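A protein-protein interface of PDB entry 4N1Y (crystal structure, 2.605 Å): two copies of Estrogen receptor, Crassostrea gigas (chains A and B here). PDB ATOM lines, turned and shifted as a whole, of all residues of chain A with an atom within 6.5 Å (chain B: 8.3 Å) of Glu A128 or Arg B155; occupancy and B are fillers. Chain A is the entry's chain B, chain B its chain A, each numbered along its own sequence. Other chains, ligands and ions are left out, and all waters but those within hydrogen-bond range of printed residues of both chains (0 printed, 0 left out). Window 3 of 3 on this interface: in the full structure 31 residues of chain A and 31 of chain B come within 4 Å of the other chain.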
ATOM      1  N   ALA A  87      -6.576  -4.720   0.349  1.00  0.00           N
ATOM      2  CA  ALA A  87      -6.696  -4.671  -1.104  1.00  0.00           C
ATOM      3  C   ALA A  87      -6.470  -3.256  -1.617  1.00  0.00           C
ATOM      4  O   ALA A  87      -5.779  -3.049  -2.611  1.00  0.00           O
ATOM      5  CB  ALA A  87      -8.056  -5.185  -1.551  1.00  0.00           C
ATOM      6  N   SER A  90      -3.131  -2.034  -1.382  1.00  0.00           N
ATOM      7  CA  SER A  90      -2.274  -2.784  -2.285  1.00  0.00           C
ATOM      8  C   SER A  90      -2.504  -2.480  -3.762  1.00  0.00           C
ATOM      9  O   SER A  90      -1.923  -3.135  -4.631  1.00  0.00           O
ATOM     10  CB  SER A  90      -2.436  -4.279  -2.025  1.00  0.00           C
ATOM     11  OG  SER A  90      -1.969  -4.588  -0.720  1.00  0.00           O
ATOM     12  N   ILE A  91      -3.356  -1.497  -4.038  1.00  0.00           N
ATOM     13  CA  ILE A  91      -3.773  -1.187  -5.404  1.00  0.00           C
ATOM     14  C   ILE A  91      -2.617  -0.925  -6.378  1.00  0.00           C
ATOM     15  O   ILE A  91      -2.692  -1.340  -7.534  1.00  0.00           O
ATOM     16  CB  ILE A  91      -4.693   0.071  -5.428  1.00  0.00           C
ATOM     17  CG1 ILE A  91      -6.112  -0.282  -5.017  1.00  0.00           C
ATOM     18  CG2 ILE A  91      -4.723   0.734  -6.810  1.00  0.00           C
ATOM     19  CD1 ILE A  91      -7.083   0.796  -5.372  1.00  0.00           C
ATOM     20  N   GLY A  94      -0.649  -3.824  -8.345  1.00  0.00           N
ATOM     21  CA  GLY A  94      -1.341  -4.543  -9.401  1.00  0.00           C
ATOM     22  C   GLY A  94      -1.358  -6.040  -9.197  1.00  0.00           C
ATOM     23  O   GLY A  94      -0.954  -6.800 -10.091  1.00  0.00           O
ATOM     24  N   GLY A  95      -1.723  -6.460  -7.985  1.00  0.00           N
ATOM     25  CA  GLY A  95      -1.891  -7.875  -7.707  1.00  0.00           C
ATOM     26  C   GLY A  95      -0.573  -8.616  -7.511  1.00  0.00           C
ATOM     27  O   GLY A  95      -0.545  -9.839  -7.414  1.00  0.00           O
ATOM     28  N   VAL A 123      -7.698 -11.906  -2.566  1.00  0.00           N
ATOM     29  CA  VAL A 123      -7.549 -10.504  -2.196  1.00  0.00           C
ATOM     30  C   VAL A 123      -6.742  -9.712  -3.195  1.00  0.00           C
ATOM     31  O   VAL A 123      -7.165  -8.648  -3.632  1.00  0.00           O
ATOM     32  CB  VAL A 123      -6.880 -10.346  -0.821  1.00  0.00           C
ATOM     33  CG1 VAL A 123      -6.663  -8.876  -0.523  1.00  0.00           C
ATOM     34  CG2 VAL A 123      -7.737 -10.986   0.258  1.00  0.00           C
ATOM     35  N   ALA A 124      -5.566 -10.235  -3.537  1.00  0.00           N
ATOM     36  CA  ALA A 124      -4.686  -9.618  -4.526  1.00  0.00           C
ATOM     37  C   ALA A 124      -5.402  -9.376  -5.869  1.00  0.00           C
ATOM     38  O   ALA A 124      -5.234  -8.318  -6.487  1.00  0.00           O
ATOM     39  CB  ALA A 124      -3.471 -10.479  -4.731  1.00  0.00           C
ATOM     40  N   ALA A 125      -6.206 -10.351  -6.304  1.00  0.00           N
ATOM     41  CA  ALA A 125      -6.987 -10.213  -7.532  1.00  0.00           C
ATOM     42  C   ALA A 125      -8.031  -9.112  -7.384  1.00  0.00           C
ATOM     43  O   ALA A 125      -8.246  -8.319  -8.299  1.00  0.00           O
ATOM     44  CB  ALA A 125      -7.667 -11.534  -7.892  1.00  0.00           C
ATOM     45  N   VAL A 126      -8.679  -9.070  -6.225  1.00  0.00           N
ATOM     46  CA  VAL A 126      -9.629  -8.016  -5.948  1.00  0.00           C
ATOM     47  C   VAL A 126      -8.906  -6.679  -6.040  1.00  0.00           C
ATOM     48  O   VAL A 126      -9.428  -5.733  -6.637  1.00  0.00           O
ATOM     49  CB  VAL A 126     -10.291  -8.180  -4.557  1.00  0.00           C
ATOM     50  CG1 VAL A 126     -10.874  -6.866  -4.089  1.00  0.00           C
ATOM     51  CG2 VAL A 126     -11.361  -9.285  -4.577  1.00  0.00           C
ATOM     52  N   SER A 127      -7.698  -6.614  -5.475  1.00  0.00           N
ATOM     53  CA  SER A 127      -6.878  -5.408  -5.564  1.00  0.00           C
ATOM     54  C   SER A 127      -6.700  -4.947  -7.014  1.00  0.00           C
ATOM     55  O   SER A 127      -6.934  -3.775  -7.341  1.00  0.00           O
ATOM     56  CB  SER A 127      -5.511  -5.636  -4.932  1.00  0.00           C
ATOM     57  OG  SER A 127      -4.809  -4.410  -4.796  1.00  0.00           O
ATOM     58  N   GLU A 128      -6.359  -5.891  -7.887  1.00  0.00           N
ATOM     59  CA  GLU A 128      -6.177  -5.588  -9.290  1.00  0.00           C
ATOM     60  C   GLU A 128      -7.453  -5.053  -9.927  1.00  0.00           C
ATOM     61  O   GLU A 128      -7.412  -4.146 -10.766  1.00  0.00           O
ATOM     62  CB  GLU A 128      -5.751  -6.826 -10.060  1.00  0.00           C
ATOM     63  CG  GLU A 128      -5.128  -6.473 -11.391  1.00  0.00           C
ATOM     64  CD  GLU A 128      -4.993  -7.663 -12.299  1.00  0.00           C
ATOM     65  OE1 GLU A 128      -5.098  -8.803 -11.801  1.00  0.00           O
ATOM     66  OE2 GLU A 128      -4.782  -7.453 -13.515  1.00  0.00           O
ATOM     67  N   GLN A 129      -8.589  -5.609  -9.525  1.00  0.00           N
ATOM     68  CA  GLN A 129      -9.852  -5.147 -10.058  1.00  0.00           C
ATOM     69  C   GLN A 129     -10.144  -3.724  -9.625  1.00  0.00           C
ATOM     70  O   GLN A 129     -10.648  -2.923 -10.421  1.00  0.00           O
ATOM     71  CB  GLN A 129     -10.977  -6.070  -9.639  1.00  0.00           C
ATOM     72  CG  GLN A 129     -10.795  -7.450 -10.178  1.00  0.00           C
ATOM     73  CD  GLN A 129     -10.765  -7.470 -11.672  1.00  0.00           C
ATOM     74  OE1 GLN A 129     -11.532  -6.766 -12.324  1.00  0.00           O
ATOM     75  NE2 GLN A 129      -9.866  -8.272 -12.238  1.00  0.00           N
ATOM     76  N   MET A 130      -9.794  -3.398  -8.386  1.00  0.00           N
ATOM     77  CA  MET A 130      -9.982  -2.037  -7.895  1.00  0.00           C
ATOM     78  C   MET A 130      -9.130  -1.076  -8.709  1.00  0.00           C
ATOM     79  O   MET A 130      -9.569   0.023  -9.061  1.00  0.00           O
ATOM     80  CB  MET A 130      -9.636  -1.931  -6.420  1.00  0.00           C
ATOM     81  CG  MET A 130     -10.496  -2.792  -5.508  1.00  0.00           C
ATOM     82  SD  MET A 130      -9.833  -2.673  -3.827  1.00  0.00           S
ATOM     83  CE  MET A 130     -11.261  -3.031  -2.822  1.00  0.00           C
ATOM     84  N   MET A 131      -7.894  -1.487  -8.967  1.00  0.00           N
ATOM     85  CA  MET A 131      -6.979  -0.713  -9.797  1.00  0.00           C
ATOM     86  C   MET A 131      -7.586  -0.500 -11.172  1.00  0.00           C
ATOM     87  O   MET A 131      -7.570   0.595 -11.708  1.00  0.00           O
ATOM     88  CB  MET A 131      -5.617  -1.412  -9.919  1.00  0.00           C
ATOM     89  CG  MET A 131      -4.649  -0.692 -10.833  1.00  0.00           C
ATOM     90  SD  MET A 131      -3.212  -1.664 -11.330  1.00  0.00           S
ATOM     91  CE  MET A 131      -3.993  -2.824 -12.462  1.00  0.00           C
ATOM     92  N   GLN A 132      -8.106  -1.572 -11.749  1.00  0.00           N
ATOM     93  CA  GLN A 132      -8.682  -1.507 -13.078  1.00  0.00           C
ATOM     94  C   GLN A 132      -9.953  -0.660 -13.140  1.00  0.00           C
ATOM     95  O   GLN A 132     -10.237  -0.048 -14.163  1.00  0.00           O
ATOM     96  CB  GLN A 132      -8.967  -2.919 -13.578  1.00  0.00           C
ATOM     97  CG  GLN A 132      -7.704  -3.690 -13.933  1.00  0.00           C
ATOM     98  CD  GLN A 132      -7.999  -5.002 -14.624  1.00  0.00           C
ATOM     99  OE1 GLN A 132      -8.747  -5.836 -14.108  1.00  0.00           O
ATOM    100  NE2 GLN A 132      -7.410  -5.197 -15.797  1.00  0.00           N
ATOM    101  N   ASN A 133     -10.714  -0.616 -12.048  1.00  0.00           N
ATOM    102  CA  ASN A 133     -11.927   0.193 -12.006  1.00  0.00           C
ATOM    103  C   ASN A 133     -11.705   1.617 -11.519  1.00  0.00           C
ATOM    104  O   ASN A 133     -12.661   2.347 -11.261  1.00  0.00           O
ATOM    105  CB  ASN A 133     -12.969  -0.475 -11.137  1.00  0.00           C
ATOM    106  CG  ASN A 133     -13.594  -1.644 -11.818  1.00  0.00           C
ATOM    107  OD1 ASN A 133     -14.368  -1.478 -12.761  1.00  0.00           O
ATOM    108  ND2 ASN A 133     -13.260  -2.848 -11.361  1.00  0.00           N
ATOM    109  N   ASP B  69     -12.105 -23.839 -18.316  1.00  0.00           N
ATOM    110  CA  ASP B  69     -12.659 -22.746 -17.540  1.00  0.00           C
ATOM    111  C   ASP B  69     -14.163 -22.948 -17.336  1.00  0.00           C
ATOM    112  O   ASP B  69     -14.686 -22.645 -16.265  1.00  0.00           O
ATOM    113  CB  ASP B  69     -12.345 -21.407 -18.207  1.00  0.00           C
ATOM    114  CG  ASP B  69     -10.864 -21.020 -18.079  1.00  0.00           C
ATOM    115  OD1 ASP B  69     -10.173 -21.581 -17.198  1.00  0.00           O
ATOM    116  OD2 ASP B  69     -10.383 -20.159 -18.858  1.00  0.00           O
ATOM    117  N   HIS B  72     -14.297 -25.199 -14.485  1.00  0.00           N
ATOM    118  CA  HIS B  72     -13.886 -24.514 -13.262  1.00  0.00           C
ATOM    119  C   HIS B  72     -14.968 -23.584 -12.710  1.00  0.00           C
ATOM    120  O   HIS B  72     -15.212 -23.570 -11.504  1.00  0.00           O
ATOM    121  CB  HIS B  72     -12.622 -23.707 -13.513  1.00  0.00           C
ATOM    122  CG  HIS B  72     -12.174 -22.903 -12.333  1.00  0.00           C
ATOM    123  ND1 HIS B  72     -11.414 -23.434 -11.315  1.00  0.00           N
ATOM    124  CD2 HIS B  72     -12.384 -21.603 -12.009  1.00  0.00           C
ATOM    125  CE1 HIS B  72     -11.165 -22.492 -10.420  1.00  0.00           C
ATOM    126  NE2 HIS B  72     -11.742 -21.372 -10.818  1.00  0.00           N
ATOM    127  N   GLU B 152     -15.210 -16.954 -10.239  1.00  0.00           N
ATOM    128  CA  GLU B 152     -13.795 -16.893  -9.934  1.00  0.00           C
ATOM    129  C   GLU B 152     -13.251 -15.516 -10.248  1.00  0.00           C
ATOM    130  O   GLU B 152     -13.389 -15.036 -11.364  1.00  0.00           O
ATOM    131  CB  GLU B 152     -13.040 -17.964 -10.737  1.00  0.00           C
ATOM    132  CG  GLU B 152     -11.549 -17.784 -10.699  1.00  0.00           C
ATOM    133  CD  GLU B 152     -10.949 -18.011  -9.329  1.00  0.00           C
ATOM    134  OE1 GLU B 152     -10.699 -17.013  -8.611  1.00  0.00           O
ATOM    135  OE2 GLU B 152     -10.748 -19.189  -8.961  1.00  0.00           O
ATOM    136  N   VAL B 153     -12.559 -14.925  -9.284  1.00  0.00           N
ATOM    137  CA  VAL B 153     -11.986 -13.590  -9.444  1.00  0.00           C
ATOM    138  C   VAL B 153     -10.507 -13.642  -9.836  1.00  0.00           C
ATOM    139  O   VAL B 153      -9.937 -12.643 -10.270  1.00  0.00           O
ATOM    140  CB  VAL B 153     -12.115 -12.769  -8.144  1.00  0.00           C
ATOM    141  CG1 VAL B 153     -11.124 -13.273  -7.092  1.00  0.00           C
ATOM    142  CG2 VAL B 153     -11.876 -11.293  -8.419  1.00  0.00           C
ATOM    143  N   ARG B 154      -9.868 -14.789  -9.629  1.00  0.00           N
ATOM    144  CA  ARG B 154      -8.496 -14.991 -10.084  1.00  0.00           C
ATOM    145  C   ARG B 154      -8.479 -15.098 -11.615  1.00  0.00           C
ATOM    146  O   ARG B 154      -9.485 -15.412 -12.246  1.00  0.00           O
ATOM    147  CB  ARG B 154      -7.883 -16.234  -9.445  1.00  0.00           C
ATOM    148  CG  ARG B 154      -7.652 -16.084  -7.952  1.00  0.00           C
ATOM    149  CD  ARG B 154      -7.156 -17.354  -7.377  1.00  0.00           C
ATOM    150  NE  ARG B 154      -8.067 -18.436  -7.724  1.00  0.00           N
ATOM    151  CZ  ARG B 154      -7.852 -19.713  -7.428  1.00  0.00           C
ATOM    152  NH1 ARG B 154      -6.739 -20.065  -6.786  1.00  0.00           N
ATOM    153  NH2 ARG B 154      -8.740 -20.635  -7.792  1.00  0.00           N
ATOM    154  N   ARG B 155      -7.327 -14.835 -12.210  1.00  0.00           N
ATOM    155  CA  ARG B 155      -7.219 -14.830 -13.658  1.00  0.00           C
ATOM    156  C   ARG B 155      -7.249 -16.222 -14.263  1.00  0.00           C
ATOM    157  O   ARG B 155      -6.442 -17.053 -13.925  1.00  0.00           O
ATOM    158  CB  ARG B 155      -5.940 -14.097 -14.018  1.00  0.00           C
ATOM    159  CG  ARG B 155      -6.087 -12.612 -14.008  1.00  0.00           C
ATOM    160  CD  ARG B 155      -4.754 -11.990 -14.166  1.00  0.00           C
ATOM    161  NE  ARG B 155      -4.852 -10.559 -14.419  1.00  0.00           N
ATOM    162  CZ  ARG B 155      -5.246 -10.049 -15.583  1.00  0.00           C
ATOM    163  NH1 ARG B 155      -5.566 -10.855 -16.586  1.00  0.00           N
ATOM    164  NH2 ARG B 155      -5.306  -8.740 -15.756  1.00  0.00           N
ATOM    165  N   LEU B 156      -8.209 -16.482 -15.140  1.00  0.00           N
ATOM    166  CA  LEU B 156      -8.248 -17.742 -15.874  1.00  0.00           C
ATOM    167  C   LEU B 156      -7.802 -17.522 -17.327  1.00  0.00           C
ATOM    168  O   LEU B 156      -7.764 -16.393 -17.810  1.00  0.00           O
ATOM    169  CB  LEU B 156      -9.646 -18.344 -15.853  1.00  0.00           C
ATOM    170  CG  LEU B 156     -10.272 -18.744 -14.521  1.00  0.00           C
ATOM    171  CD1 LEU B 156     -11.736 -19.078 -14.760  1.00  0.00           C
ATOM    172  CD2 LEU B 156      -9.542 -19.903 -13.870  1.00  0.00           C
ATOM    173  N   ALA B 157      -7.511 -18.604 -18.033  1.00  0.00           N
ATOM    174  CA  ALA B 157      -7.138 -18.514 -19.432  1.00  0.00           C
ATOM    175  C   ALA B 157      -8.156 -17.699 -20.250  1.00  0.00           C
ATOM    176  O   ALA B 157      -7.784 -16.910 -21.132  1.00  0.00           O
ATOM    177  CB  ALA B 157      -6.983 -19.911 -20.009  1.00  0.00           C
ATOM    178  N   SER B 158      -9.437 -17.884 -19.965  1.00  0.00           N
ATOM    179  CA  SER B 158     -10.471 -17.198 -20.739  1.00  0.00           C
ATOM    180  C   SER B 158     -10.823 -15.833 -20.172  1.00  0.00           C
ATOM    181  O   SER B 158     -11.929 -15.333 -20.408  1.00  0.00           O
ATOM    182  CB  SER B 158     -11.732 -18.045 -20.838  1.00  0.00           C
ATOM    183  OG  SER B 158     -11.469 -19.286 -21.465  1.00  0.00           O
ATOM    184  N   TYR B 159      -9.884 -15.239 -19.434  1.00  0.00           N
ATOM    185  CA  TYR B 159     -10.108 -13.970 -18.751  1.00  0.00           C
ATOM    186  C   TYR B 159     -10.768 -12.951 -19.665  1.00  0.00           C
ATOM    187  O   TYR B 159     -11.785 -12.349 -19.327  1.00  0.00           O
ATOM    188  CB  TYR B 159      -8.797 -13.422 -18.247  1.00  0.00           C
ATOM    189  CG  TYR B 159      -8.863 -12.087 -17.542  1.00  0.00           C
ATOM    190  CD1 TYR B 159      -9.200 -12.003 -16.184  1.00  0.00           C
ATOM    191  CD2 TYR B 159      -8.564 -10.917 -18.218  1.00  0.00           C
ATOM    192  CE1 TYR B 159      -9.224 -10.788 -15.528  1.00  0.00           C
ATOM    193  CE2 TYR B 159      -8.604  -9.692 -17.577  1.00  0.00           C
ATOM    194  CZ  TYR B 159      -8.935  -9.632 -16.239  1.00  0.00           C
ATOM    195  OH  TYR B 159      -8.963  -8.404 -15.622  1.00  0.00           O
ATOM    196  N   ASN B 160     -10.201 -12.791 -20.844  1.00  0.00           N
ATOM    197  CA  ASN B 160     -10.724 -11.841 -21.793  1.00  0.00           C
ATOM    198  C   ASN B 160     -12.211 -12.045 -22.098  1.00  0.00           C
ATOM    199  O   ASN B 160     -13.016 -11.094 -22.060  1.00  0.00           O
ATOM    200  CB  ASN B 160      -9.930 -11.917 -23.082  1.00  0.00           C
ATOM    201  CG  ASN B 160     -10.352 -10.861 -24.053  1.00  0.00           C
ATOM    202  OD1 ASN B 160     -10.708 -11.164 -25.190  1.00  0.00           O
ATOM    203  ND2 ASN B 160     -10.350  -9.605 -23.604  1.00  0.00           N
ATOM    204  N   ILE B 162     -14.467 -13.960 -20.385  1.00  0.00           N
ATOM    205  CA  ILE B 162     -15.265 -13.844 -19.181  1.00  0.00           C
ATOM    206  C   ILE B 162     -15.551 -12.382 -18.897  1.00  0.00           C
ATOM    207  O   ILE B 162     -16.660 -12.017 -18.498  1.00  0.00           O
ATOM    208  CB  ILE B 162     -14.575 -14.487 -17.965  1.00  0.00           C
ATOM    209  CG1 ILE B 162     -14.476 -16.002 -18.158  1.00  0.00           C
ATOM    210  CG2 ILE B 162     -15.374 -14.224 -16.698  1.00  0.00           C
ATOM    211  CD1 ILE B 162     -13.568 -16.681 -17.156  1.00  0.00           C
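Printed residues of chain B within 4 Å of Ala A125: Val B153 (3.5 Å). Glu A128 touches one residue of chain B. Of the printed residues of chain B, Gln A129 touches Tyr B159 (3.5 Å). Of the printed residues of chain A, Val B153 touches Ala A125. Of chain A, only Glu A128 comes within 4 Å of Arg B155. Leu B156 touches none of the printed residues of chain A. Of the printed residues of chain A, Tyr B159 touches Gln A129 and Gln A132. The nearest residue of chain A that does not touch Arg B155 is Gln A132 (4.1 Å). The nearest printed residue of chain B that does not touch Gln A129 is Val B153 (4.4 Å).
OE1 of Gln A132 is in hydrogen-bond range of NE2 of Gln A129 (3.3 Å). The backbone carbonyl oxygen (O) of Gln A129 lies within hydrogen-bond range of the side-chain amide nitrogen (ND2) of Asn A133, 2.8 Å away.
No position is printed for both chains. Of the 4 pairs that touch across the chains among the printed residues, none has its exchanged pair printed and touching as well.
Printed residues of chain A that touch a printed residue of chain B: Ala A125, Glu A128, Gln A129 and Gln A132. Hydrophobic or aromatic side chains of chain A within 4 Å of the printed part of chain B: Ala A125. Among the printed residues, Asp or Glu carboxylates within 4 Å of a Lys or Arg side-chain nitrogen of the other chain: Glu A128 with Arg B155 (2.6 Å).
The guanidinium group of Arg B155 is in salt-bridge range of the side-chain carboxylate of Glu A128 (2.6 Å). The side-chain hydroxyl (OH) of Tyr B159 is in hydrogen-bond range of the side-chain amide oxygen (OE1) of Gln A132 (3.0 Å).
Ala A125 touches Val B153. Gln A129 touches Tyr B159.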
